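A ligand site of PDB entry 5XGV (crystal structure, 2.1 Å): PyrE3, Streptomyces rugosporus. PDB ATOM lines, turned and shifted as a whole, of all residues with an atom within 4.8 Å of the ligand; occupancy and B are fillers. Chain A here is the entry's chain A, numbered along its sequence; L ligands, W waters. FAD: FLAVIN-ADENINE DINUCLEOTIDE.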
ATOM      1  N   GLY A   8       6.680 -15.024  26.196  1.00  0.00           N
ATOM      2  CA  GLY A   8       6.090 -15.304  24.906  1.00  0.00           C
ATOM      3  C   GLY A   8       5.446 -14.088  24.284  1.00  0.00           C
ATOM      4  O   GLY A   8       4.612 -13.432  24.901  1.00  0.00           O
ATOM      5  N   GLY A   9       5.820 -13.780  23.055  1.00  0.00           N
ATOM      6  CA  GLY A   9       5.243 -12.658  22.338  1.00  0.00           C
ATOM      7  C   GLY A   9       4.432 -13.089  21.131  1.00  0.00           C
ATOM      8  O   GLY A   9       4.552 -12.508  20.063  1.00  0.00           O
ATOM      9  N   GLY A  10       3.652 -14.141  21.286  1.00  0.00           N
ATOM     10  CA  GLY A  10       2.636 -14.486  20.308  1.00  0.00           C
ATOM     11  C   GLY A  10       1.468 -13.528  20.464  1.00  0.00           C
ATOM     12  O   GLY A  10       1.577 -12.538  21.180  1.00  0.00           O
ATOM     13  N   PRO A  11       0.341 -13.819  19.794  1.00  0.00           N
ATOM     14  CA  PRO A  11      -0.815 -12.910  19.865  1.00  0.00           C
ATOM     15  C   PRO A  11      -1.346 -12.699  21.299  1.00  0.00           C
ATOM     16  O   PRO A  11      -1.744 -11.597  21.661  1.00  0.00           O
ATOM     17  CB  PRO A  11      -1.885 -13.610  19.019  1.00  0.00           C
ATOM     18  CG  PRO A  11      -1.192 -14.714  18.303  1.00  0.00           C
ATOM     19  CD  PRO A  11       0.062 -15.037  19.013  1.00  0.00           C
ATOM     20  N   VAL A  12      -1.378 -13.761  22.102  1.00  0.00           N
ATOM     21  CA  VAL A  12      -1.891 -13.661  23.456  1.00  0.00           C
ATOM     22  C   VAL A  12      -0.951 -12.852  24.364  1.00  0.00           C
ATOM     23  O   VAL A  12      -1.383 -11.933  25.072  1.00  0.00           O
ATOM     24  CB  VAL A  12      -2.144 -15.073  24.049  1.00  0.00           C
ATOM     25  CG1 VAL A  12      -2.675 -14.967  25.486  1.00  0.00           C
ATOM     26  CG2 VAL A  12      -3.144 -15.856  23.165  1.00  0.00           C
ATOM     27  N   GLY A  13       0.347 -13.177  24.335  1.00  0.00           N
ATOM     28  CA  GLY A  13       1.323 -12.390  25.065  1.00  0.00           C
ATOM     29  C   GLY A  13       1.292 -10.915  24.673  1.00  0.00           C
ATOM     30  O   GLY A  13       1.299 -10.033  25.525  1.00  0.00           O
ATOM     31  N   LEU A  30       9.294 -11.284  26.748  1.00  0.00           N
ATOM     32  CA  LEU A  30      10.435 -12.048  26.297  1.00  0.00           C
ATOM     33  C   LEU A  30       9.955 -13.009  25.227  1.00  0.00           C
ATOM     34  O   LEU A  30       9.064 -13.819  25.465  1.00  0.00           O
ATOM     35  CB  LEU A  30      11.069 -12.789  27.458  1.00  0.00           C
ATOM     36  CG  LEU A  30      11.372 -11.895  28.667  1.00  0.00           C
ATOM     37  CD1 LEU A  30      11.922 -12.719  29.826  1.00  0.00           C
ATOM     38  CD2 LEU A  30      12.347 -10.782  28.290  1.00  0.00           C
ATOM     39  N   GLU A  31      10.530 -12.886  24.028  1.00  0.00           N
ATOM     40  CA  GLU A  31      10.102 -13.669  22.893  1.00  0.00           C
ATOM     41  C   GLU A  31      11.290 -14.243  22.144  1.00  0.00           C
ATOM     42  O   GLU A  31      12.263 -13.557  21.881  1.00  0.00           O
ATOM     43  CB  GLU A  31       9.248 -12.814  21.945  1.00  0.00           C
ATOM     44  CG  GLU A  31       9.085 -13.395  20.550  1.00  0.00           C
ATOM     45  CD  GLU A  31       8.383 -14.748  20.532  1.00  0.00           C
ATOM     46  OE1 GLU A  31       8.792 -15.600  19.730  1.00  0.00           O
ATOM     47  OE2 GLU A  31       7.420 -14.954  21.309  1.00  0.00           O
ATOM     48  N   ARG A  32      11.177 -15.522  21.773  1.00  0.00           N
ATOM     49  CA  ARG A  32      12.265 -16.267  21.175  1.00  0.00           C
ATOM     50  C   ARG A  32      12.622 -15.764  19.771  1.00  0.00           C
ATOM     51  O   ARG A  32      13.780 -15.585  19.454  1.00  0.00           O
ATOM     52  CB  ARG A  32      11.896 -17.745  21.153  1.00  0.00           C
ATOM     53  CG  ARG A  32      12.386 -18.559  20.008  1.00  0.00           C
ATOM     54  CD  ARG A  32      11.687 -19.924  20.031  1.00  0.00           C
ATOM     55  NE  ARG A  32      11.946 -20.645  21.283  1.00  0.00           N
ATOM     56  CZ  ARG A  32      11.051 -21.409  21.908  1.00  0.00           C
ATOM     57  NH1 ARG A  32       9.812 -21.545  21.415  1.00  0.00           N
ATOM     58  NH2 ARG A  32      11.382 -22.035  23.024  1.00  0.00           N
ATOM     59  N   HIS A  33      11.608 -15.494  18.958  1.00  0.00           N
ATOM     60  CA  HIS A  33      11.849 -15.153  17.554  1.00  0.00           C
ATOM     61  C   HIS A  33      12.187 -13.681  17.309  1.00  0.00           C
ATOM     62  O   HIS A  33      11.786 -12.792  18.059  1.00  0.00           O
ATOM     63  CB  HIS A  33      10.629 -15.550  16.744  1.00  0.00           C
ATOM     64  CG  HIS A  33      10.369 -17.017  16.732  1.00  0.00           C
ATOM     65  ND1 HIS A  33       9.162 -17.565  17.082  1.00  0.00           N
ATOM     66  CD2 HIS A  33      11.190 -18.059  16.442  1.00  0.00           C
ATOM     67  CE1 HIS A  33       9.231 -18.883  16.992  1.00  0.00           C
ATOM     68  NE2 HIS A  33      10.452 -19.207  16.612  1.00  0.00           N
ATOM     69  N   ARG A  41      -0.135 -19.464  10.896  1.00  0.00           N
ATOM     70  CA  ARG A  41      -0.949 -20.649  11.058  1.00  0.00           C
ATOM     71  C   ARG A  41      -2.415 -20.337  10.773  1.00  0.00           C
ATOM     72  O   ARG A  41      -3.126 -21.132  10.162  1.00  0.00           O
ATOM     73  CB  ARG A  41      -0.762 -21.220  12.463  1.00  0.00           C
ATOM     74  CG  ARG A  41       0.710 -21.413  12.794  1.00  0.00           C
ATOM     75  CD  ARG A  41       0.999 -21.213  14.274  1.00  0.00           C
ATOM     76  NE  ARG A  41       0.357 -22.224  15.096  1.00  0.00           N
ATOM     77  CZ  ARG A  41       0.383 -22.208  16.435  1.00  0.00           C
ATOM     78  NH1 ARG A  41      -0.223 -23.166  17.121  1.00  0.00           N
ATOM     79  NH2 ARG A  41       1.005 -21.227  17.065  1.00  0.00           N
ATOM     80  N   GLY A  42      -2.844 -19.162  11.222  1.00  0.00           N
ATOM     81  CA  GLY A  42      -4.220 -18.733  11.068  1.00  0.00           C
ATOM     82  C   GLY A  42      -4.388 -17.578  10.101  1.00  0.00           C
ATOM     83  O   GLY A  42      -3.480 -16.758   9.924  1.00  0.00           O
ATOM     84  N   GLY A  43      -5.563 -17.520   9.465  1.00  0.00           N
ATOM     85  CA  GLY A  43      -5.860 -16.474   8.520  1.00  0.00           C
ATOM     86  C   GLY A  43      -7.135 -15.708   8.819  1.00  0.00           C
ATOM     87  O   GLY A  43      -7.585 -14.904   8.024  1.00  0.00           O
ATOM     88  N   ALA A  44      -7.740 -15.956   9.976  1.00  0.00           N
ATOM     89  CA  ALA A  44      -8.937 -15.220  10.361  1.00  0.00           C
ATOM     90  C   ALA A  44      -9.062 -15.082  11.867  1.00  0.00           C
ATOM     91  O   ALA A  44      -8.479 -15.862  12.629  1.00  0.00           O
ATOM     92  CB  ALA A  44     -10.177 -15.888   9.813  1.00  0.00           C
ATOM     93  N   HIS A  96      -2.397 -14.065  10.934  1.00  0.00           N
ATOM     94  CA  HIS A  96      -2.098 -13.813  12.334  1.00  0.00           C
ATOM     95  C   HIS A  96      -0.754 -13.126  12.551  1.00  0.00           C
ATOM     96  O   HIS A  96      -0.570 -12.432  13.544  1.00  0.00           O
ATOM     97  CB  HIS A  96      -2.155 -15.117  13.137  1.00  0.00           C
ATOM     98  CG  HIS A  96      -3.548 -15.639  13.318  1.00  0.00           C
ATOM     99  ND1 HIS A  96      -3.859 -16.676  14.175  1.00  0.00           N
ATOM    100  CD2 HIS A  96      -4.726 -15.274  12.747  1.00  0.00           C
ATOM    101  CE1 HIS A  96      -5.149 -16.925  14.118  1.00  0.00           C
ATOM    102  NE2 HIS A  96      -5.698 -16.082  13.265  1.00  0.00           N
ATOM    103  N   THR A 118      15.027 -13.644  22.475  1.00  0.00           N
ATOM    104  CA  THR A 118      15.342 -14.028  23.849  1.00  0.00           C
ATOM    105  C   THR A 118      14.741 -15.388  24.197  1.00  0.00           C
ATOM    106  O   THR A 118      13.525 -15.574  24.134  1.00  0.00           O
ATOM    107  CB  THR A 118      14.831 -12.949  24.850  1.00  0.00           C
ATOM    108  OG1 THR A 118      15.317 -11.655  24.453  1.00  0.00           O
ATOM    109  CG2 THR A 118      15.310 -13.250  26.256  1.00  0.00           C
ATOM    110  N   GLU A 119      15.613 -16.341  24.534  1.00  0.00           N
ATOM    111  CA  GLU A 119      15.203 -17.678  24.959  1.00  0.00           C
ATOM    112  C   GLU A 119      15.068 -17.716  26.466  1.00  0.00           C
ATOM    113  O   GLU A 119      16.043 -17.541  27.161  1.00  0.00           O
ATOM    114  CB  GLU A 119      16.231 -18.760  24.560  1.00  0.00           C
ATOM    115  CG  GLU A 119      15.949 -19.542  23.292  1.00  0.00           C
ATOM    116  CD  GLU A 119      14.652 -20.324  23.306  1.00  0.00           C
ATOM    117  OE1 GLU A 119      14.357 -21.044  24.289  1.00  0.00           O
ATOM    118  OE2 GLU A 119      13.916 -20.214  22.326  1.00  0.00           O
ATOM    119  N   ILE A 120      13.868 -17.956  26.970  1.00  0.00           N
ATOM    120  CA  ILE A 120      13.745 -18.226  28.382  1.00  0.00           C
ATOM    121  C   ILE A 120      14.175 -19.659  28.641  1.00  0.00           C
ATOM    122  O   ILE A 120      13.747 -20.576  27.928  1.00  0.00           O
ATOM    123  CB  ILE A 120      12.321 -18.026  28.878  1.00  0.00           C
ATOM    124  CG1 ILE A 120      11.914 -16.569  28.729  1.00  0.00           C
ATOM    125  CG2 ILE A 120      12.196 -18.510  30.336  1.00  0.00           C
ATOM    126  CD1 ILE A 120      10.461 -16.360  28.931  1.00  0.00           C
ATOM    127  N   CYS A 148       2.660 -16.984  28.478  1.00  0.00           N
ATOM    128  CA  CYS A 148       1.981 -16.948  27.190  1.00  0.00           C
ATOM    129  C   CYS A 148       2.893 -17.599  26.146  1.00  0.00           C
ATOM    130  O   CYS A 148       3.017 -17.127  24.995  1.00  0.00           O
ATOM    131  CB  CYS A 148       1.634 -15.489  26.800  1.00  0.00           C
ATOM    132  SG  CYS A 148       0.690 -14.542  28.070  1.00  0.00           S
ATOM    133  N   ASP A 149       3.541 -18.693  26.557  1.00  0.00           N
ATOM    134  CA  ASP A 149       4.608 -19.271  25.755  1.00  0.00           C
ATOM    135  C   ASP A 149       4.171 -20.517  24.979  1.00  0.00           C
ATOM    136  O   ASP A 149       4.971 -21.396  24.718  1.00  0.00           O
ATOM    137  CB  ASP A 149       5.850 -19.603  26.619  1.00  0.00           C
ATOM    138  CG  ASP A 149       5.505 -20.361  27.911  1.00  0.00           C
ATOM    139  OD1 ASP A 149       4.333 -20.378  28.356  1.00  0.00           O
ATOM    140  OD2 ASP A 149       6.452 -20.906  28.522  1.00  0.00           O
ATOM    141  N   GLY A 150       2.895 -20.562  24.608  1.00  0.00           N
ATOM    142  CA  GLY A 150       2.417 -21.585  23.692  1.00  0.00           C
ATOM    143  C   GLY A 150       2.074 -22.942  24.268  1.00  0.00           C
ATOM    144  O   GLY A 150       2.189 -23.193  25.468  1.00  0.00           O
ATOM    145  N   SER A 151       1.740 -23.833  23.373  1.00  0.00           N
ATOM    146  CA  SER A 151       1.268 -25.148  23.692  1.00  0.00           C
ATOM    147  C   SER A 151       2.256 -25.988  24.508  1.00  0.00           C
ATOM    148  O   SER A 151       1.872 -26.670  25.383  1.00  0.00           O
ATOM    149  CB  SER A 151       0.873 -25.894  22.427  1.00  0.00           C
ATOM    150  OG  SER A 151      -0.346 -25.453  21.931  1.00  0.00           O
ATOM    151  N   LEU A 154       6.996 -23.855  28.700  1.00  0.00           N
ATOM    152  CA  LEU A 154       8.008 -24.034  29.677  1.00  0.00           C
ATOM    153  C   LEU A 154       7.545 -23.513  31.024  1.00  0.00           C
ATOM    154  O   LEU A 154       7.801 -24.140  32.014  1.00  0.00           O
ATOM    155  CB  LEU A 154       9.269 -23.380  29.211  1.00  0.00           C
ATOM    156  CG  LEU A 154      10.485 -23.384  30.098  1.00  0.00           C
ATOM    157  CD1 LEU A 154      11.737 -23.103  29.277  1.00  0.00           C
ATOM    158  CD2 LEU A 154      10.341 -22.411  31.226  1.00  0.00           C
ATOM    159  N   TRP A 174      -0.240 -29.499   7.159  1.00  0.00           N
ATOM    160  CA  TRP A 174      -0.497 -28.210   6.550  1.00  0.00           C
ATOM    161  C   TRP A 174       0.758 -27.604   5.951  1.00  0.00           C
ATOM    162  O   TRP A 174       1.879 -27.899   6.356  1.00  0.00           O
ATOM    163  CB  TRP A 174      -1.149 -27.234   7.539  1.00  0.00           C
ATOM    164  CG  TRP A 174      -0.272 -26.633   8.608  1.00  0.00           C
ATOM    165  CD1 TRP A 174       0.034 -27.195   9.811  1.00  0.00           C
ATOM    166  CD2 TRP A 174       0.358 -25.338   8.591  1.00  0.00           C
ATOM    167  NE1 TRP A 174       0.838 -26.343  10.536  1.00  0.00           N
ATOM    168  CE2 TRP A 174       1.053 -25.200   9.814  1.00  0.00           C
ATOM    169  CE3 TRP A 174       0.415 -24.299   7.659  1.00  0.00           C
ATOM    170  CZ2 TRP A 174       1.788 -24.063  10.121  1.00  0.00           C
ATOM    171  CZ3 TRP A 174       1.140 -23.170   7.973  1.00  0.00           C
ATOM    172  CH2 TRP A 174       1.817 -23.059   9.194  1.00  0.00           C
ATOM    173  N   TRP A 254       0.246 -31.054  12.471  1.00  0.00           N
ATOM    174  CA  TRP A 254      -0.490 -30.497  13.587  1.00  0.00           C
ATOM    175  C   TRP A 254      -1.311 -31.602  14.198  1.00  0.00           C
ATOM    176  O   TRP A 254      -1.528 -32.651  13.577  1.00  0.00           O
ATOM    177  CB  TRP A 254      -1.378 -29.316  13.162  1.00  0.00           C
ATOM    178  CG  TRP A 254      -2.373 -29.597  12.089  1.00  0.00           C
ATOM    179  CD1 TRP A 254      -2.115 -29.848  10.778  1.00  0.00           C
ATOM    180  CD2 TRP A 254      -3.811 -29.606  12.223  1.00  0.00           C
ATOM    181  NE1 TRP A 254      -3.288 -30.032  10.084  1.00  0.00           N
ATOM    182  CE2 TRP A 254      -4.339 -29.888  10.949  1.00  0.00           C
ATOM    183  CE3 TRP A 254      -4.683 -29.418  13.296  1.00  0.00           C
ATOM    184  CZ2 TRP A 254      -5.718 -29.990  10.718  1.00  0.00           C
ATOM    185  CZ3 TRP A 254      -6.045 -29.506  13.063  1.00  0.00           C
ATOM    186  CH2 TRP A 254      -6.545 -29.792  11.794  1.00  0.00           C
ATOM    187  N   ALA A 272      -1.749 -18.086  30.262  1.00  0.00           N
ATOM    188  CA  ALA A 272      -2.759 -17.569  29.317  1.00  0.00           C
ATOM    189  C   ALA A 272      -2.563 -18.151  27.916  1.00  0.00           C
ATOM    190  O   ALA A 272      -1.466 -18.555  27.557  1.00  0.00           O
ATOM    191  CB  ALA A 272      -2.708 -16.011  29.269  1.00  0.00           C
ATOM    192  N   GLY A 273      -3.624 -18.196  27.130  1.00  0.00           N
ATOM    193  CA  GLY A 273      -3.517 -18.674  25.769  1.00  0.00           C
ATOM    194  C   GLY A 273      -3.265 -20.176  25.663  1.00  0.00           C
ATOM    195  O   GLY A 273      -3.731 -20.950  26.491  1.00  0.00           O
ATOM    196  N   ASP A 274      -2.520 -20.577  24.637  1.00  0.00           N
ATOM    197  CA  ASP A 274      -2.250 -22.001  24.364  1.00  0.00           C
ATOM    198  C   ASP A 274      -1.541 -22.681  25.551  1.00  0.00           C
ATOM    199  O   ASP A 274      -1.729 -23.872  25.785  1.00  0.00           O
ATOM    200  CB  ASP A 274      -1.430 -22.163  23.072  1.00  0.00           C
ATOM    201  CG  ASP A 274      -2.306 -22.149  21.803  1.00  0.00           C
ATOM    202  OD1 ASP A 274      -3.486 -21.742  21.875  1.00  0.00           O
ATOM    203  OD2 ASP A 274      -1.808 -22.530  20.719  1.00  0.00           O
ATOM    204  N   ALA A 275      -0.746 -21.930  26.288  1.00  0.00           N
ATOM    205  CA  ALA A 275      -0.117 -22.470  27.494  1.00  0.00           C
ATOM    206  C   ALA A 275      -1.168 -22.934  28.486  1.00  0.00           C
ATOM    207  O   ALA A 275      -0.966 -23.925  29.197  1.00  0.00           O
ATOM    208  CB  ALA A 275       0.787 -21.438  28.136  1.00  0.00           C
ATOM    209  N   PRO A 281      -7.816 -26.353  16.484  1.00  0.00           N
ATOM    210  CA  PRO A 281      -7.886 -25.069  15.750  1.00  0.00           C
ATOM    211  C   PRO A 281      -8.992 -24.974  14.681  1.00  0.00           C
ATOM    212  O   PRO A 281      -8.815 -25.369  13.522  1.00  0.00           O
ATOM    213  CB  PRO A 281      -6.502 -24.965  15.116  1.00  0.00           C
ATOM    214  CG  PRO A 281      -5.927 -26.337  15.118  1.00  0.00           C
ATOM    215  CD  PRO A 281      -6.581 -27.106  16.242  1.00  0.00           C
ATOM    216  N   GLY A 284     -11.985 -20.362  15.016  1.00  0.00           N
ATOM    217  CA  GLY A 284     -11.461 -19.206  15.703  1.00  0.00           C
ATOM    218  C   GLY A 284     -11.538 -19.236  17.216  1.00  0.00           C
ATOM    219  O   GLY A 284     -11.058 -18.322  17.855  1.00  0.00           O
ATOM    220  N   GLN A 285     -12.118 -20.282  17.798  1.00  0.00           N
ATOM    221  CA  GLN A 285     -12.141 -20.419  19.263  1.00  0.00           C
ATOM    222  C   GLN A 285     -10.759 -20.656  19.880  1.00  0.00           C
ATOM    223  O   GLN A 285     -10.530 -20.315  21.052  1.00  0.00           O
ATOM    224  CB  GLN A 285     -13.094 -21.554  19.660  1.00  0.00           C
ATOM    225  CG  GLN A 285     -14.567 -21.125  19.653  1.00  0.00           C
ATOM    226  CD  GLN A 285     -15.526 -22.260  19.975  1.00  0.00           C
ATOM    227  OE1 GLN A 285     -15.857 -23.072  19.113  1.00  0.00           O
ATOM    228  NE2 GLN A 285     -15.962 -22.320  21.206  1.00  0.00           N
ATOM    229  N   ALA A 286      -9.839 -21.229  19.117  1.00  0.00           N
ATOM    230  CA  ALA A 286      -8.512 -21.518  19.651  1.00  0.00           C
ATOM    231  C   ALA A 286      -7.806 -20.215  20.030  1.00  0.00           C
ATOM    232  O   ALA A 286      -7.346 -20.057  21.167  1.00  0.00           O
ATOM    233  CB  ALA A 286      -7.684 -22.309  18.674  1.00  0.00           C
ATOM    234  N   LEU A 287      -7.711 -19.286  19.088  1.00  0.00           N
ATOM    235  CA  LEU A 287      -7.112 -17.990  19.416  1.00  0.00           C
ATOM    236  C   LEU A 287      -8.048 -17.138  20.287  1.00  0.00           C
ATOM    237  O   LEU A 287      -7.612 -16.518  21.249  1.00  0.00           O
ATOM    238  CB  LEU A 287      -6.729 -17.215  18.161  1.00  0.00           C
ATOM    239  CG  LEU A 287      -6.217 -15.790  18.397  1.00  0.00           C
ATOM    240  CD1 LEU A 287      -4.998 -15.781  19.342  1.00  0.00           C
ATOM    241  CD2 LEU A 287      -5.890 -15.097  17.082  1.00  0.00           C
ATOM    242  N   GLY A 288      -9.340 -17.119  19.931  1.00  0.00           N
ATOM    243  CA  GLY A 288     -10.325 -16.323  20.655  1.00  0.00           C
ATOM    244  C   GLY A 288     -10.283 -16.514  22.164  1.00  0.00           C
ATOM    245  O   GLY A 288     -10.269 -15.526  22.909  1.00  0.00           O
HETATM  246  PA  FAD L   1       1.688 -18.875  20.349  1.00  0.00           P
HETATM  247  O1A FAD L   1       2.211 -20.282  20.232  1.00  0.00           O
HETATM  248  O2A FAD L   1       1.054 -18.236  19.159  1.00  0.00           O
HETATM  249  O5B FAD L   1       2.857 -17.928  20.895  1.00  0.00           O
HETATM  250  C5B FAD L   1       3.728 -18.372  21.922  1.00  0.00           C
HETATM  251  C4B FAD L   1       5.033 -17.603  21.799  1.00  0.00           C
HETATM  252  O4B FAD L   1       5.910 -17.952  22.854  1.00  0.00           O
HETATM  253  C3B FAD L   1       5.765 -17.981  20.508  1.00  0.00           C
HETATM  254  O3B FAD L   1       6.049 -16.783  19.807  1.00  0.00           O
HETATM  255  C2B FAD L   1       7.052 -18.649  20.956  1.00  0.00           C
HETATM  256  O2B FAD L   1       8.123 -18.257  20.099  1.00  0.00           O
HETATM  257  C1B FAD L   1       7.227 -18.083  22.350  1.00  0.00           C
HETATM  258  N9A FAD L   1       7.978 -18.969  23.253  1.00  0.00           N
HETATM  259  C8A FAD L   1       7.638 -20.217  23.614  1.00  0.00           C
HETATM  260  N7A FAD L   1       8.539 -20.729  24.491  1.00  0.00           N
HETATM  261  C5A FAD L   1       9.486 -19.784  24.680  1.00  0.00           C
HETATM  262  C6A FAD L   1      10.718 -19.663  25.467  1.00  0.00           C
HETATM  263  N6A FAD L   1      11.155 -20.684  26.252  1.00  0.00           N
HETATM  264  N1A FAD L   1      11.400 -18.503  25.393  1.00  0.00           N
HETATM  265  C2A FAD L   1      10.992 -17.471  24.619  1.00  0.00           C
HETATM  266  N3A FAD L   1       9.884 -17.518  23.873  1.00  0.00           N
HETATM  267  C4A FAD L   1       9.101 -18.626  23.872  1.00  0.00           C
HETATM  268  N1  FAD L   1      -6.556 -20.225  15.636  1.00  0.00           N
HETATM  269  C2  FAD L   1      -7.550 -19.489  15.089  1.00  0.00           C
HETATM  270  O2  FAD L   1      -8.155 -18.663  15.801  1.00  0.00           O
HETATM  271  N3  FAD L   1      -7.897 -19.606  13.790  1.00  0.00           N
HETATM  272  C4  FAD L   1      -7.294 -20.466  12.971  1.00  0.00           C
HETATM  273  O4  FAD L   1      -7.619 -20.572  11.777  1.00  0.00           O
HETATM  274  C4X FAD L   1      -6.196 -21.283  13.490  1.00  0.00           C
HETATM  275  N5  FAD L   1      -5.572 -22.139  12.677  1.00  0.00           N
HETATM  276  C5X FAD L   1      -4.574 -22.906  13.153  1.00  0.00           C
HETATM  277  C6  FAD L   1      -3.958 -23.790  12.288  1.00  0.00           C
HETATM  278  C7  FAD L   1      -2.925 -24.592  12.751  1.00  0.00           C
HETATM  279  C7M FAD L   1      -2.229 -25.548  11.811  1.00  0.00           C
HETATM  280  C8  FAD L   1      -2.498 -24.496  14.172  1.00  0.00           C
HETATM  281  C8M FAD L   1      -1.368 -25.362  14.652  1.00  0.00           C
HETATM  282  C9  FAD L   1      -3.121 -23.604  15.037  1.00  0.00           C
HETATM  283  C9A FAD L   1      -4.152 -22.788  14.578  1.00  0.00           C
HETATM  284  N10 FAD L   1      -4.809 -21.884  15.438  1.00  0.00           N
HETATM  285  C10 FAD L   1      -5.851 -21.110  14.900  1.00  0.00           C
HETATM  286  C1' FAD L   1      -4.461 -21.736  16.854  1.00  0.00           C
HETATM  287  C2' FAD L   1      -3.689 -20.447  17.118  1.00  0.00           C
HETATM  288  O2' FAD L   1      -2.527 -20.424  16.286  1.00  0.00           O
HETATM  289  C3' FAD L   1      -3.267 -20.371  18.585  1.00  0.00           C
HETATM  290  O3' FAD L   1      -4.446 -20.485  19.376  1.00  0.00           O
HETATM  291  C4' FAD L   1      -2.554 -19.063  18.967  1.00  0.00           C
HETATM  292  O4' FAD L   1      -1.328 -18.900  18.224  1.00  0.00           O
HETATM  293  C5' FAD L   1      -2.255 -19.039  20.463  1.00  0.00           C
HETATM  294  O5' FAD L   1      -1.487 -17.886  20.762  1.00  0.00           O
HETATM  295  P   FAD L   1      -0.466 -17.855  21.995  1.00  0.00           P
HETATM  296  O1P FAD L   1       0.101 -16.470  21.987  1.00  0.00           O
HETATM  297  O2P FAD L   1      -1.141 -18.414  23.216  1.00  0.00           O
HETATM  298  O3P FAD L   1       0.686 -18.928  21.609  1.00  0.00           O
HETATM  299  O   HOH W   1       2.149 -15.215  23.348  1.00  0.00           O
HETATM  300  O   HOH W   2       0.208 -19.147  25.289  1.00  0.00           O
HETATM  301  O   HOH W   3      -7.863 -20.226   8.676  1.00  0.00           O
HETATM  302  O   HOH W   4       4.661 -21.947  20.287  1.00  0.00           O
HETATM  303  O   HOH W   5       7.648 -22.943  25.753  1.00  0.00           O
HETATM  304  O   HOH W   6      -1.840 -17.948  15.185  1.00  0.00           O
HETATM  305  O   HOH W   7       8.954 -19.370  28.333  1.00  0.00           O
HETATM  306  O   HOH W   8      10.185 -23.382  25.526  1.00  0.00           O
HETATM  307  O   HOH W   9       1.077 -27.355  15.940  1.00  0.00           O
HETATM  308  O   HOH W  10       2.247 -17.118  17.244  1.00  0.00           O
HETATM  309  O   HOH W  11       0.992 -22.636  20.729  1.00  0.00           O
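N of His 33 sits at hydrogen-bond distance from OE1 of Glu 31, at 2.9 Å.
The side-chain carboxylate of Asp 274 lies within hydrogen-bond range of the side-chain hydroxyl of Ser 151, 3.5 Å away.
The backbone NH (N) of Leu 154 is in hydrogen-bond range of the side-chain carboxylate (OD2) of Asp 149 (3.0 Å).
The backbone NH (N) of Arg 32 sits close to the backbone carbonyl oxygen (O) of Thr 118 (3.3 Å).
O of Leu 30 sits at hydrogen-bond distance from N of Gly 8, 2.8 Å away.
O of Gly 150 lies close to N of Ala 275.
The backbone carbonyl oxygen of Gly 42 sits at hydrogen-bond distance from the backbone NH of His 96, 3.1 Å away.
A ring nitrogen (NE2) of His 96 is in hydrogen-bond range of the backbone carbonyl oxygen of Ala 44 (2.9 Å).
Water W11 lies within hydrogen-bond range of an oxygen (O1A) of the ligand (2.7 Å), the side-chain carboxylate (OD2) of Asp 274 (2.8 Å) and the backbone NH (N) of Ser 151 (3.0 Å).
Water W5 lies within hydrogen-bond range of a nitrogen (N7A) of the ligand (2.7 Å), the backbone NH of Leu 154 (3.2 Å) and the backbone carbonyl oxygen of Asp 149 (3.3 Å).
Water W1 lies within hydrogen-bond range of O of Cys 148 (2.7 Å), O1P of the ligand (2.8 Å), N of Gly 10 (2.8 Å), N of Gly 13 (2.9 Å) and O of Gly 8 (3.4 Å).
Water W6 bridges a ring nitrogen (ND1) of His 96 (2.6 Å) and an oxygen (O2') of the ligand (2.8 Å).
Water W8 bridges a nitrogen (N6A) of the ligand (3.0 Å) and the guanidinium group of Arg 32 (3.1 Å).
Water W7 bridges the side-chain carboxylate of Asp 149 (2.9 Å) and a nitrogen (N6A) of the ligand (3.3 Å).
The backbone nitrogen (N) of Pro 11 lies close to an oxygen (O1P) of the ligand, 3.4 Å away.
CA of Gly 8 touches O4B of the ligand (3.4 Å).
Gly 10 touches the ligand (CA to O5B, 3.5 Å).
CA of Gly 42 touches O4 of the ligand, at 3.9 Å.
Ala 44 touches the ligand.
His 96 touches the ligand.
O of Thr 118 touches C2A of the ligand, at 3.2 Å.
Glu 119 touches the ligand.
O of Cys 148 touches C5B of the ligand (3.4 Å).
O of Asp 149 touches C8A of the ligand, 3.1 Å away.
Gly 150 touches the ligand.
Leu 154 touches the ligand.
Trp 174 touches the ligand (NE1 to C7M, 3.4 Å).
Gly 273 touches the ligand.
Pro 281 touches the ligand.
Gly 284 touches the ligand (CA to O2, 3.4 Å).
Hydrophobic or aromatic side chains that line the ligand: Pro 11, Val 12, His 33, His 96, Ile 120, Leu 154, Trp 174, Pro 281, Ala 286 and Leu 287.
Of the 35 residues printed, 25 come within 4 Å of the ligand.
The nearest printed residue that does not touch the ligand is Gly 13 (4.1 Å).
An oxygen (O3B) of the ligand lies within hydrogen-bond range of the side-chain carboxylate (OE2) of Glu 31, 2.7 Å away.
N of Asp 274 lies within hydrogen-bond range of O2P of the ligand, 2.9 Å away.
The side-chain carboxylate (OD1) of Asp 274 is in hydrogen-bond range of an oxygen (O3') of the ligand, at 3.0 Å.
The backbone NH of Ile 120 sits at hydrogen-bond distance from a nitrogen (N1A) of the ligand, 3.0 Å away.
O of Ile 120 sits at hydrogen-bond distance from N6A of the ligand.
N of Val 12 sits at hydrogen-bond distance from O1P of the ligand (3.1 Å).
O2 of the ligand lies close to N of Leu 287 (3.4 Å).
A nitrogen (N3A) of the ligand sits at hydrogen-bond distance from the backbone NH (N) of Arg 32, 3.2 Å away.
The guanidinium group (NH1) of Arg 32 sits close to a nitrogen (N7A) of the ligand, 3.4 Å away.
An oxygen (O2B) of the ligand lies within hydrogen-bond range of a ring nitrogen (ND1) of His 33, 3.3 Å away.
O1A of the ligand lies within salt-bridge range of NH2 of Arg 41 (3.5 Å).
The backbone carbonyl oxygen of Ala 286 sits close to an oxygen (O3') of the ligand, at 3.4 Å.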
